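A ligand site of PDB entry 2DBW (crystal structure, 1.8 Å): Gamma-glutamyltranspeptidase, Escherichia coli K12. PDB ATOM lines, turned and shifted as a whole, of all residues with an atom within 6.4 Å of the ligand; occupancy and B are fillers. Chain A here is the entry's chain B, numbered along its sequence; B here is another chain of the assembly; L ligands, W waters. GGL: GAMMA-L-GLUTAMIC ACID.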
ATOM      1  N   THR A   1      25.949  -5.307  28.041  1.00  0.00           N
ATOM      2  CA  THR A   1      26.629  -4.285  28.827  1.00  0.00           C
ATOM      3  C   THR A   1      26.140  -4.318  30.269  1.00  0.00           C
ATOM      4  O   THR A   1      25.008  -4.728  30.531  1.00  0.00           O
ATOM      5  CB  THR A   1      26.358  -2.867  28.294  1.00  0.00           C
ATOM      6  OG1 THR A   1      26.721  -2.794  26.898  1.00  0.00           O
ATOM      7  CG2 THR A   1      27.162  -1.824  29.075  1.00  0.00           C
ATOM      8  N   THR A   2      26.982  -3.884  31.190  1.00  0.00           N
ATOM      9  CA  THR A   2      26.603  -3.827  32.587  1.00  0.00           C
ATOM     10  C   THR A   2      27.395  -2.696  33.250  1.00  0.00           C
ATOM     11  O   THR A   2      28.534  -2.417  32.875  1.00  0.00           O
ATOM     12  CB  THR A   2      26.861  -5.178  33.321  1.00  0.00           C
ATOM     13  OG1 THR A   2      26.200  -5.155  34.595  1.00  0.00           O
ATOM     14  CG2 THR A   2      28.362  -5.412  33.539  1.00  0.00           C
ATOM     15  N   THR A  17      31.590   0.753  33.427  1.00  0.00           N
ATOM     16  CA  THR A  17      30.625   0.201  32.472  1.00  0.00           C
ATOM     17  C   THR A  17      31.491  -0.629  31.527  1.00  0.00           C
ATOM     18  O   THR A  17      32.435  -0.106  30.953  1.00  0.00           O
ATOM     19  CB  THR A  17      29.921   1.280  31.611  1.00  0.00           C
ATOM     20  OG1 THR A  17      29.387   2.319  32.431  1.00  0.00           O
ATOM     21  CG2 THR A  17      28.766   0.638  30.827  1.00  0.00           C
ATOM     22  N   TYR A  18      31.205  -1.919  31.410  1.00  0.00           N
ATOM     23  CA  TYR A  18      31.977  -2.715  30.452  1.00  0.00           C
ATOM     24  C   TYR A  18      31.052  -3.711  29.800  1.00  0.00           C
ATOM     25  O   TYR A  18      29.929  -3.929  30.280  1.00  0.00           O
ATOM     26  CB  TYR A  18      33.227  -3.359  31.088  1.00  0.00           C
ATOM     27  CG  TYR A  18      33.048  -4.497  32.065  1.00  0.00           C
ATOM     28  CD1 TYR A  18      34.094  -5.395  32.268  1.00  0.00           C
ATOM     29  CD2 TYR A  18      31.873  -4.675  32.792  1.00  0.00           C
ATOM     30  CE1 TYR A  18      33.979  -6.448  33.167  1.00  0.00           C
ATOM     31  CE2 TYR A  18      31.744  -5.733  33.695  1.00  0.00           C
ATOM     32  CZ  TYR A  18      32.800  -6.615  33.872  1.00  0.00           C
ATOM     33  OH  TYR A  18      32.697  -7.682  34.743  1.00  0.00           O
ATOM     34  N   THR A  19      31.485  -4.316  28.698  1.00  0.00           N
ATOM     35  CA  THR A  19      30.559  -5.164  27.957  1.00  0.00           C
ATOM     36  C   THR A  19      31.193  -6.065  26.904  1.00  0.00           C
ATOM     37  O   THR A  19      32.367  -5.935  26.567  1.00  0.00           O
ATOM     38  CB  THR A  19      29.573  -4.221  27.240  1.00  0.00           C
ATOM     39  OG1 THR A  19      28.646  -4.963  26.444  1.00  0.00           O
ATOM     40  CG2 THR A  19      30.344  -3.260  26.331  1.00  0.00           C
ATOM     41  N   LEU A  20      30.382  -7.002  26.395  1.00  0.00           N
ATOM     42  CA  LEU A  20      30.763  -7.916  25.315  1.00  0.00           C
ATOM     43  C   LEU A  20      30.000  -7.384  24.093  1.00  0.00           C
ATOM     44  O   LEU A  20      30.129  -7.904  22.991  1.00  0.00           O
ATOM     45  CB  LEU A  20      30.281  -9.331  25.599  1.00  0.00           C
ATOM     46  CG  LEU A  20      31.026 -10.187  26.617  1.00  0.00           C
ATOM     47  CD1 LEU A  20      30.307 -11.509  26.794  1.00  0.00           C
ATOM     48  CD2 LEU A  20      32.459 -10.403  26.141  1.00  0.00           C
ATOM     49  N   ASN A  21      29.229  -6.334  24.352  1.00  0.00           N
ATOM     50  CA  ASN A  21      28.330  -5.640  23.434  1.00  0.00           C
ATOM     51  C   ASN A  21      26.956  -6.279  23.621  1.00  0.00           C
ATOM     52  O   ASN A  21      26.307  -6.015  24.623  1.00  0.00           O
ATOM     53  CB  ASN A  21      28.755  -5.710  21.959  1.00  0.00           C
ATOM     54  CG  ASN A  21      27.824  -4.898  21.052  1.00  0.00           C
ATOM     55  OD1 ASN A  21      27.116  -4.018  21.529  1.00  0.00           O
ATOM     56  ND2 ASN A  21      27.837  -5.188  19.761  1.00  0.00           N
ATOM     57  N   THR A  22      26.515  -7.132  22.691  1.00  0.00           N
ATOM     58  CA  THR A  22      25.199  -7.756  22.879  1.00  0.00           C
ATOM     59  C   THR A  22      25.305  -8.816  23.971  1.00  0.00           C
ATOM     60  O   THR A  22      26.397  -9.153  24.422  1.00  0.00           O
ATOM     61  CB  THR A  22      24.653  -8.379  21.559  1.00  0.00           C
ATOM     62  OG1 THR A  22      25.446  -9.512  21.187  1.00  0.00           O
ATOM     63  CG2 THR A  22      24.679  -7.357  20.445  1.00  0.00           C
ATOM     64  N   GLN A  40      31.966  -6.407  19.579  1.00  0.00           N
ATOM     65  CA  GLN A  40      32.076  -4.940  19.612  1.00  0.00           C
ATOM     66  C   GLN A  40      32.279  -4.306  18.240  1.00  0.00           C
ATOM     67  O   GLN A  40      32.024  -3.113  18.069  1.00  0.00           O
ATOM     68  CB  GLN A  40      33.222  -4.525  20.531  1.00  0.00           C
ATOM     69  CG  GLN A  40      32.886  -3.353  21.450  1.00  0.00           C
ATOM     70  CD  GLN A  40      31.933  -3.762  22.567  1.00  0.00           C
ATOM     71  OE1 GLN A  40      30.847  -3.188  22.702  1.00  0.00           O
ATOM     72  NE2 GLN A  40      32.329  -4.749  23.348  1.00  0.00           N
ATOM     73  N   ASP A  43      29.898  -1.883  16.561  1.00  0.00           N
ATOM     74  CA  ASP A  43      29.762  -0.493  16.994  1.00  0.00           C
ATOM     75  C   ASP A  43      30.405   0.471  15.996  1.00  0.00           C
ATOM     76  O   ASP A  43      30.205   1.676  16.080  1.00  0.00           O
ATOM     77  CB  ASP A  43      30.376  -0.276  18.386  1.00  0.00           C
ATOM     78  CG  ASP A  43      29.434  -0.723  19.494  1.00  0.00           C
ATOM     79  OD1 ASP A  43      28.224  -0.910  19.232  1.00  0.00           O
ATOM     80  OD2 ASP A  43      29.897  -0.872  20.653  1.00  0.00           O
ATOM     81  N   TYR A  54      21.854  -0.968  17.135  1.00  0.00           N
ATOM     82  CA  TYR A  54      21.159  -0.013  17.995  1.00  0.00           C
ATOM     83  C   TYR A  54      20.507   1.127  17.225  1.00  0.00           C
ATOM     84  O   TYR A  54      19.966   2.054  17.829  1.00  0.00           O
ATOM     85  CB  TYR A  54      22.137   0.568  19.029  1.00  0.00           C
ATOM     86  CG  TYR A  54      22.771  -0.494  19.890  1.00  0.00           C
ATOM     87  CD1 TYR A  54      22.007  -1.267  20.769  1.00  0.00           C
ATOM     88  CD2 TYR A  54      24.138  -0.768  19.787  1.00  0.00           C
ATOM     89  CE1 TYR A  54      22.579  -2.295  21.516  1.00  0.00           C
ATOM     90  CE2 TYR A  54      24.720  -1.792  20.544  1.00  0.00           C
ATOM     91  CZ  TYR A  54      23.935  -2.548  21.397  1.00  0.00           C
ATOM     92  OH  TYR A  54      24.501  -3.584  22.112  1.00  0.00           O
ATOM     93  N   LEU A  56      22.105   3.174  15.324  1.00  0.00           N
ATOM     94  CA  LEU A  56      23.062   4.262  15.211  1.00  0.00           C
ATOM     95  C   LEU A  56      23.724   4.241  13.834  1.00  0.00           C
ATOM     96  O   LEU A  56      23.935   3.180  13.247  1.00  0.00           O
ATOM     97  CB  LEU A  56      24.137   4.153  16.295  1.00  0.00           C
ATOM     98  CG  LEU A  56      23.643   4.321  17.734  1.00  0.00           C
ATOM     99  CD1 LEU A  56      24.750   3.954  18.713  1.00  0.00           C
ATOM    100  CD2 LEU A  56      23.168   5.750  17.964  1.00  0.00           C
ATOM    101  N   PRO A  70      36.201   1.172  18.222  1.00  0.00           N
ATOM    102  CA  PRO A  70      34.867   1.550  17.766  1.00  0.00           C
ATOM    103  C   PRO A  70      34.177   2.499  18.745  1.00  0.00           C
ATOM    104  O   PRO A  70      34.349   2.378  19.959  1.00  0.00           O
ATOM    105  CB  PRO A  70      34.134   0.220  17.647  1.00  0.00           C
ATOM    106  CG  PRO A  70      34.813  -0.637  18.678  1.00  0.00           C
ATOM    107  CD  PRO A  70      36.275  -0.273  18.500  1.00  0.00           C
ATOM    108  N   LEU A  71      33.417   3.444  18.214  1.00  0.00           N
ATOM    109  CA  LEU A  71      32.714   4.414  19.038  1.00  0.00           C
ATOM    110  C   LEU A  71      31.745   3.731  20.000  1.00  0.00           C
ATOM    111  O   LEU A  71      31.025   2.808  19.631  1.00  0.00           O
ATOM    112  CB  LEU A  71      31.945   5.396  18.151  1.00  0.00           C
ATOM    113  CG  LEU A  71      31.238   6.544  18.889  1.00  0.00           C
ATOM    114  CD1 LEU A  71      32.278   7.478  19.512  1.00  0.00           C
ATOM    115  CD2 LEU A  71      30.357   7.295  17.915  1.00  0.00           C
ATOM    116  N   SER A  72      31.726   4.216  21.242  1.00  0.00           N
ATOM    117  CA  SER A  72      30.836   3.660  22.257  1.00  0.00           C
ATOM    118  C   SER A  72      29.878   4.725  22.758  1.00  0.00           C
ATOM    119  O   SER A  72      30.042   5.913  22.461  1.00  0.00           O
ATOM    120  CB  SER A  72      31.662   3.127  23.429  1.00  0.00           C
ATOM    121  OG  SER A  72      30.818   2.630  24.461  1.00  0.00           O
ATOM    122  N   SER A  73      28.861   4.297  23.499  1.00  0.00           N
ATOM    123  CA  SER A  73      27.893   5.204  24.083  1.00  0.00           C
ATOM    124  C   SER A  73      27.963   5.067  25.600  1.00  0.00           C
ATOM    125  O   SER A  73      27.242   5.756  26.326  1.00  0.00           O
ATOM    126  CB  SER A  73      26.463   4.877  23.615  1.00  0.00           C
ATOM    127  OG  SER A  73      26.314   5.044  22.214  1.00  0.00           O
ATOM    128  N   MET A  74      28.820   4.159  26.078  1.00  0.00           N
ATOM    129  CA  MET A  74      28.946   3.933  27.512  1.00  0.00           C
ATOM    130  C   MET A  74      29.282   5.204  28.260  1.00  0.00           C
ATOM    131  O   MET A  74      30.164   5.973  27.863  1.00  0.00           O
ATOM    132  CB  MET A  74      29.983   2.840  27.788  1.00  0.00           C
ATOM    133  CG  MET A  74      29.491   1.472  27.343  1.00  0.00           C
ATOM    134  SD  MET A  74      30.647   0.045  27.900  1.00  0.00           S
ATOM    135  CE  MET A  74      31.903   0.094  26.427  1.00  0.00           C
ATOM    136  N   SER A  91      24.923   3.102  33.140  1.00  0.00           N
ATOM    137  CA  SER A  91      23.960   2.085  32.732  1.00  0.00           C
ATOM    138  C   SER A  91      24.266   1.478  31.379  1.00  0.00           C
ATOM    139  O   SER A  91      25.052   2.031  30.594  1.00  0.00           O
ATOM    140  CB  SER A  91      22.565   2.725  32.667  1.00  0.00           C
ATOM    141  OG  SER A  91      21.615   1.874  32.030  1.00  0.00           O
ATOM    142  N   PRO A  92      23.703   0.291  31.110  1.00  0.00           N
ATOM    143  CA  PRO A  92      23.899  -0.387  29.826  1.00  0.00           C
ATOM    144  C   PRO A  92      22.746   0.135  28.968  1.00  0.00           C
ATOM    145  O   PRO A  92      21.961   0.956  29.428  1.00  0.00           O
ATOM    146  CB  PRO A  92      23.725  -1.856  30.187  1.00  0.00           C
ATOM    147  CG  PRO A  92      22.697  -1.806  31.280  1.00  0.00           C
ATOM    148  CD  PRO A  92      23.190  -0.650  32.128  1.00  0.00           C
ATOM    149  N   GLY A  93      22.637  -0.324  27.719  1.00  0.00           N
ATOM    150  CA  GLY A  93      21.542   0.121  26.883  1.00  0.00           C
ATOM    151  C   GLY A  93      21.899   0.572  25.486  1.00  0.00           C
ATOM    152  O   GLY A  93      21.088   1.186  24.794  1.00  0.00           O
ATOM    153  N   GLY A  94      23.127   0.275  25.061  1.00  0.00           N
ATOM    154  CA  GLY A  94      23.551   0.676  23.727  1.00  0.00           C
ATOM    155  C   GLY A  94      23.361   2.164  23.506  1.00  0.00           C
ATOM    156  O   GLY A  94      23.843   2.978  24.289  1.00  0.00           O
ATOM    157  N   SER A  95      22.636   2.518  22.458  1.00  0.00           N
ATOM    158  CA  SER A  95      22.387   3.924  22.149  1.00  0.00           C
ATOM    159  C   SER A  95      21.625   4.649  23.263  1.00  0.00           C
ATOM    160  O   SER A  95      21.765   5.848  23.437  1.00  0.00           O
ATOM    161  CB  SER A  95      21.609   4.046  20.838  1.00  0.00           C
ATOM    162  OG  SER A  95      20.402   3.315  20.918  1.00  0.00           O
ATOM    163  N   ILE A  97      22.040   4.425  26.471  1.00  0.00           N
ATOM    164  CA  ILE A  97      22.849   4.752  27.651  1.00  0.00           C
ATOM    165  C   ILE A  97      22.898   6.268  27.885  1.00  0.00           C
ATOM    166  O   ILE A  97      22.718   6.738  29.014  1.00  0.00           O
ATOM    167  CB  ILE A  97      24.297   4.244  27.500  1.00  0.00           C
ATOM    168  CG1 ILE A  97      24.308   2.717  27.513  1.00  0.00           C
ATOM    169  CG2 ILE A  97      25.166   4.815  28.630  1.00  0.00           C
ATOM    170  CD1 ILE A  97      25.685   2.103  27.305  1.00  0.00           C
ATOM    171  N   PHE B  74      34.898   1.061  30.023  1.00  0.00           N
ATOM    172  CA  PHE B  74      35.432   2.315  30.518  1.00  0.00           C
ATOM    173  C   PHE B  74      35.293   2.409  32.036  1.00  0.00           C
ATOM    174  O   PHE B  74      34.387   1.814  32.627  1.00  0.00           O
ATOM    175  CB  PHE B  74      34.659   3.477  29.896  1.00  0.00           C
ATOM    176  CG  PHE B  74      34.799   3.549  28.402  1.00  0.00           C
ATOM    177  CD1 PHE B  74      35.962   4.047  27.820  1.00  0.00           C
ATOM    178  CD2 PHE B  74      33.754   3.144  27.574  1.00  0.00           C
ATOM    179  CE1 PHE B  74      36.082   4.135  26.440  1.00  0.00           C
ATOM    180  CE2 PHE B  74      33.874   3.232  26.193  1.00  0.00           C
ATOM    181  CZ  PHE B  74      35.033   3.729  25.625  1.00  0.00           C
ATOM    182  N   ARG B  90      38.667   0.045  25.854  1.00  0.00           N
ATOM    183  CA  ARG B  90      37.784  -0.304  24.742  1.00  0.00           C
ATOM    184  C   ARG B  90      38.592  -1.186  23.799  1.00  0.00           C
ATOM    185  O   ARG B  90      39.795  -0.985  23.622  1.00  0.00           O
ATOM    186  CB  ARG B  90      37.363   0.975  24.027  1.00  0.00           C
ATOM    187  CG  ARG B  90      36.501   0.795  22.798  1.00  0.00           C
ATOM    188  CD  ARG B  90      35.134   0.236  23.163  1.00  0.00           C
ATOM    189  NE  ARG B  90      34.158   0.535  22.121  1.00  0.00           N
ATOM    190  CZ  ARG B  90      32.883   0.155  22.146  1.00  0.00           C
ATOM    191  NH1 ARG B  90      32.426  -0.550  23.172  1.00  0.00           N
ATOM    192  NH2 ARG B  90      32.073   0.520  21.166  1.00  0.00           N
ATOM    193  N   ARG B 313      26.417  13.206  16.771  1.00  0.00           N
ATOM    194  CA  ARG B 313      27.123  11.974  17.070  1.00  0.00           C
ATOM    195  C   ARG B 313      27.481  11.201  15.794  1.00  0.00           C
ATOM    196  O   ARG B 313      28.593  10.680  15.655  1.00  0.00           O
ATOM    197  CB  ARG B 313      26.254  11.070  17.961  1.00  0.00           C
ATOM    198  CG  ARG B 313      26.925   9.768  18.376  1.00  0.00           C
ATOM    199  CD  ARG B 313      25.966   8.881  19.166  1.00  0.00           C
ATOM    200  NE  ARG B 313      26.616   7.736  19.789  1.00  0.00           N
ATOM    201  CZ  ARG B 313      27.062   6.663  19.134  1.00  0.00           C
ATOM    202  NH1 ARG B 313      26.924   6.571  17.819  1.00  0.00           N
ATOM    203  NH2 ARG B 313      27.627   5.664  19.809  1.00  0.00           N
HETATM  204  N   GGL L   1      28.469  -1.807  22.669  1.00  0.00           N
HETATM  205  CA  GGL L   1      27.674  -0.594  22.866  1.00  0.00           C
HETATM  206  C   GGL L   1      28.553   0.603  23.212  1.00  0.00           C
HETATM  207  O   GGL L   1      27.986   1.710  23.337  1.00  0.00           O
HETATM  208  CB  GGL L   1      26.623  -0.804  23.956  1.00  0.00           C
HETATM  209  CG  GGL L   1      27.003  -1.818  25.023  1.00  0.00           C
HETATM  210  CD  GGL L   1      25.861  -2.191  26.076  1.00  0.00           C
HETATM  211  OE1 GGL L   1      25.036  -1.218  26.483  1.00  0.00           O
HETATM  212  OXT GGL L   1      29.704   0.375  23.631  1.00  0.00           O
HETATM  213  O   HOH W   1      25.971   2.338  21.585  1.00  0.00           O
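The side-chain hydroxyl (OG1) of Thr 19 lies within hydrogen-bond range of the side-chain hydroxyl (OG1) of Thr 1, at 2.9 Å.
The side-chain carboxylate of Asp 43 is in salt-bridge range of the guanidinium group of Arg 90 of chain B (2.6 Å).
The side-chain hydroxyl of Ser 72 lies within hydrogen-bond range of the backbone NH of Met 74 of chain A (3.0 Å).
The side-chain hydroxyl of Ser 73 sits at hydrogen-bond distance from the guanidinium group of Arg 313 of chain B.
The backbone NH (N) of Asn 21 sits at hydrogen-bond distance from the side-chain hydroxyl (OG1) of Thr 19 (2.6 Å).
The side-chain hydroxyl (OH) of Tyr 54 lies within hydrogen-bond range of the side-chain amide oxygen (OD1) of Asn 21, at 2.7 Å.
The backbone carbonyl oxygen (O) of Leu 71 is in hydrogen-bond range of the guanidinium group (NH2) of Arg 90 of chain B, 2.9 Å away.
The side-chain hydroxyl (OG) of Ser 95 sits at hydrogen-bond distance from the backbone carbonyl oxygen (O) of Tyr 54 (3.4 Å).
Water W1 lies within hydrogen-bond range of O of the ligand (2.7 Å), OG of Ser 73 (2.8 Å), N of Ser 95 (3.5 Å) and O of Gly 94 (3.5 Å).
A carbon (CD) of the ligand is bonded to the side-chain hydroxyl (OG1) of Thr 1 (1.3 Å).
The side-chain carboxylate (OD2) of Asp 43 lies within salt-bridge range of a nitrogen (N) of the ligand, at 2.6 Å.
The side-chain hydroxyl (OG) of Ser 72 is in hydrogen-bond range of an oxygen (OXT) of the ligand, 2.6 Å away.
The backbone NH (N) of Ser 73 is in hydrogen-bond range of an oxygen (O) of the ligand, 2.7 Å away.
A nitrogen (N) of the ligand sits at hydrogen-bond distance from the side-chain amide oxygen of Gln 40 (2.8 Å).
The backbone NH of Gly 94 lies within hydrogen-bond range of an oxygen (OE1) of the ligand.
The side-chain amide oxygen (OD1) of Asn 21 lies within hydrogen-bond range of a nitrogen (N) of the ligand, 2.8 Å away.
N of Gly 93 is in hydrogen-bond range of OE1 of the ligand (2.8 Å).
NH1 of Arg 90 of chain B lies within salt-bridge range of OXT of the ligand, at 2.9 Å.
Merely in contact with the ligand: Thr 19, Tyr 54, Met 74 of chain A, Pro 92 and Ile 97.
Hydrophobic or aromatic side chains within 4 Å of the ligand: Tyr 54, Met 74 of chain A, Pro 92 and Ile 97.
14 residues have an atom within 4 Å of the ligand: Thr 1, Thr 19, Asn 21, Gln 40, Asp 43, Tyr 54, Ser 72, Ser 73, Met 74 of chain A, Pro 92, Gly 93, Gly 94, Ile 97 and Arg 90 of chain B.
The nearest printed residue that does not touch the ligand is Leu 71 (4.9 Å).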
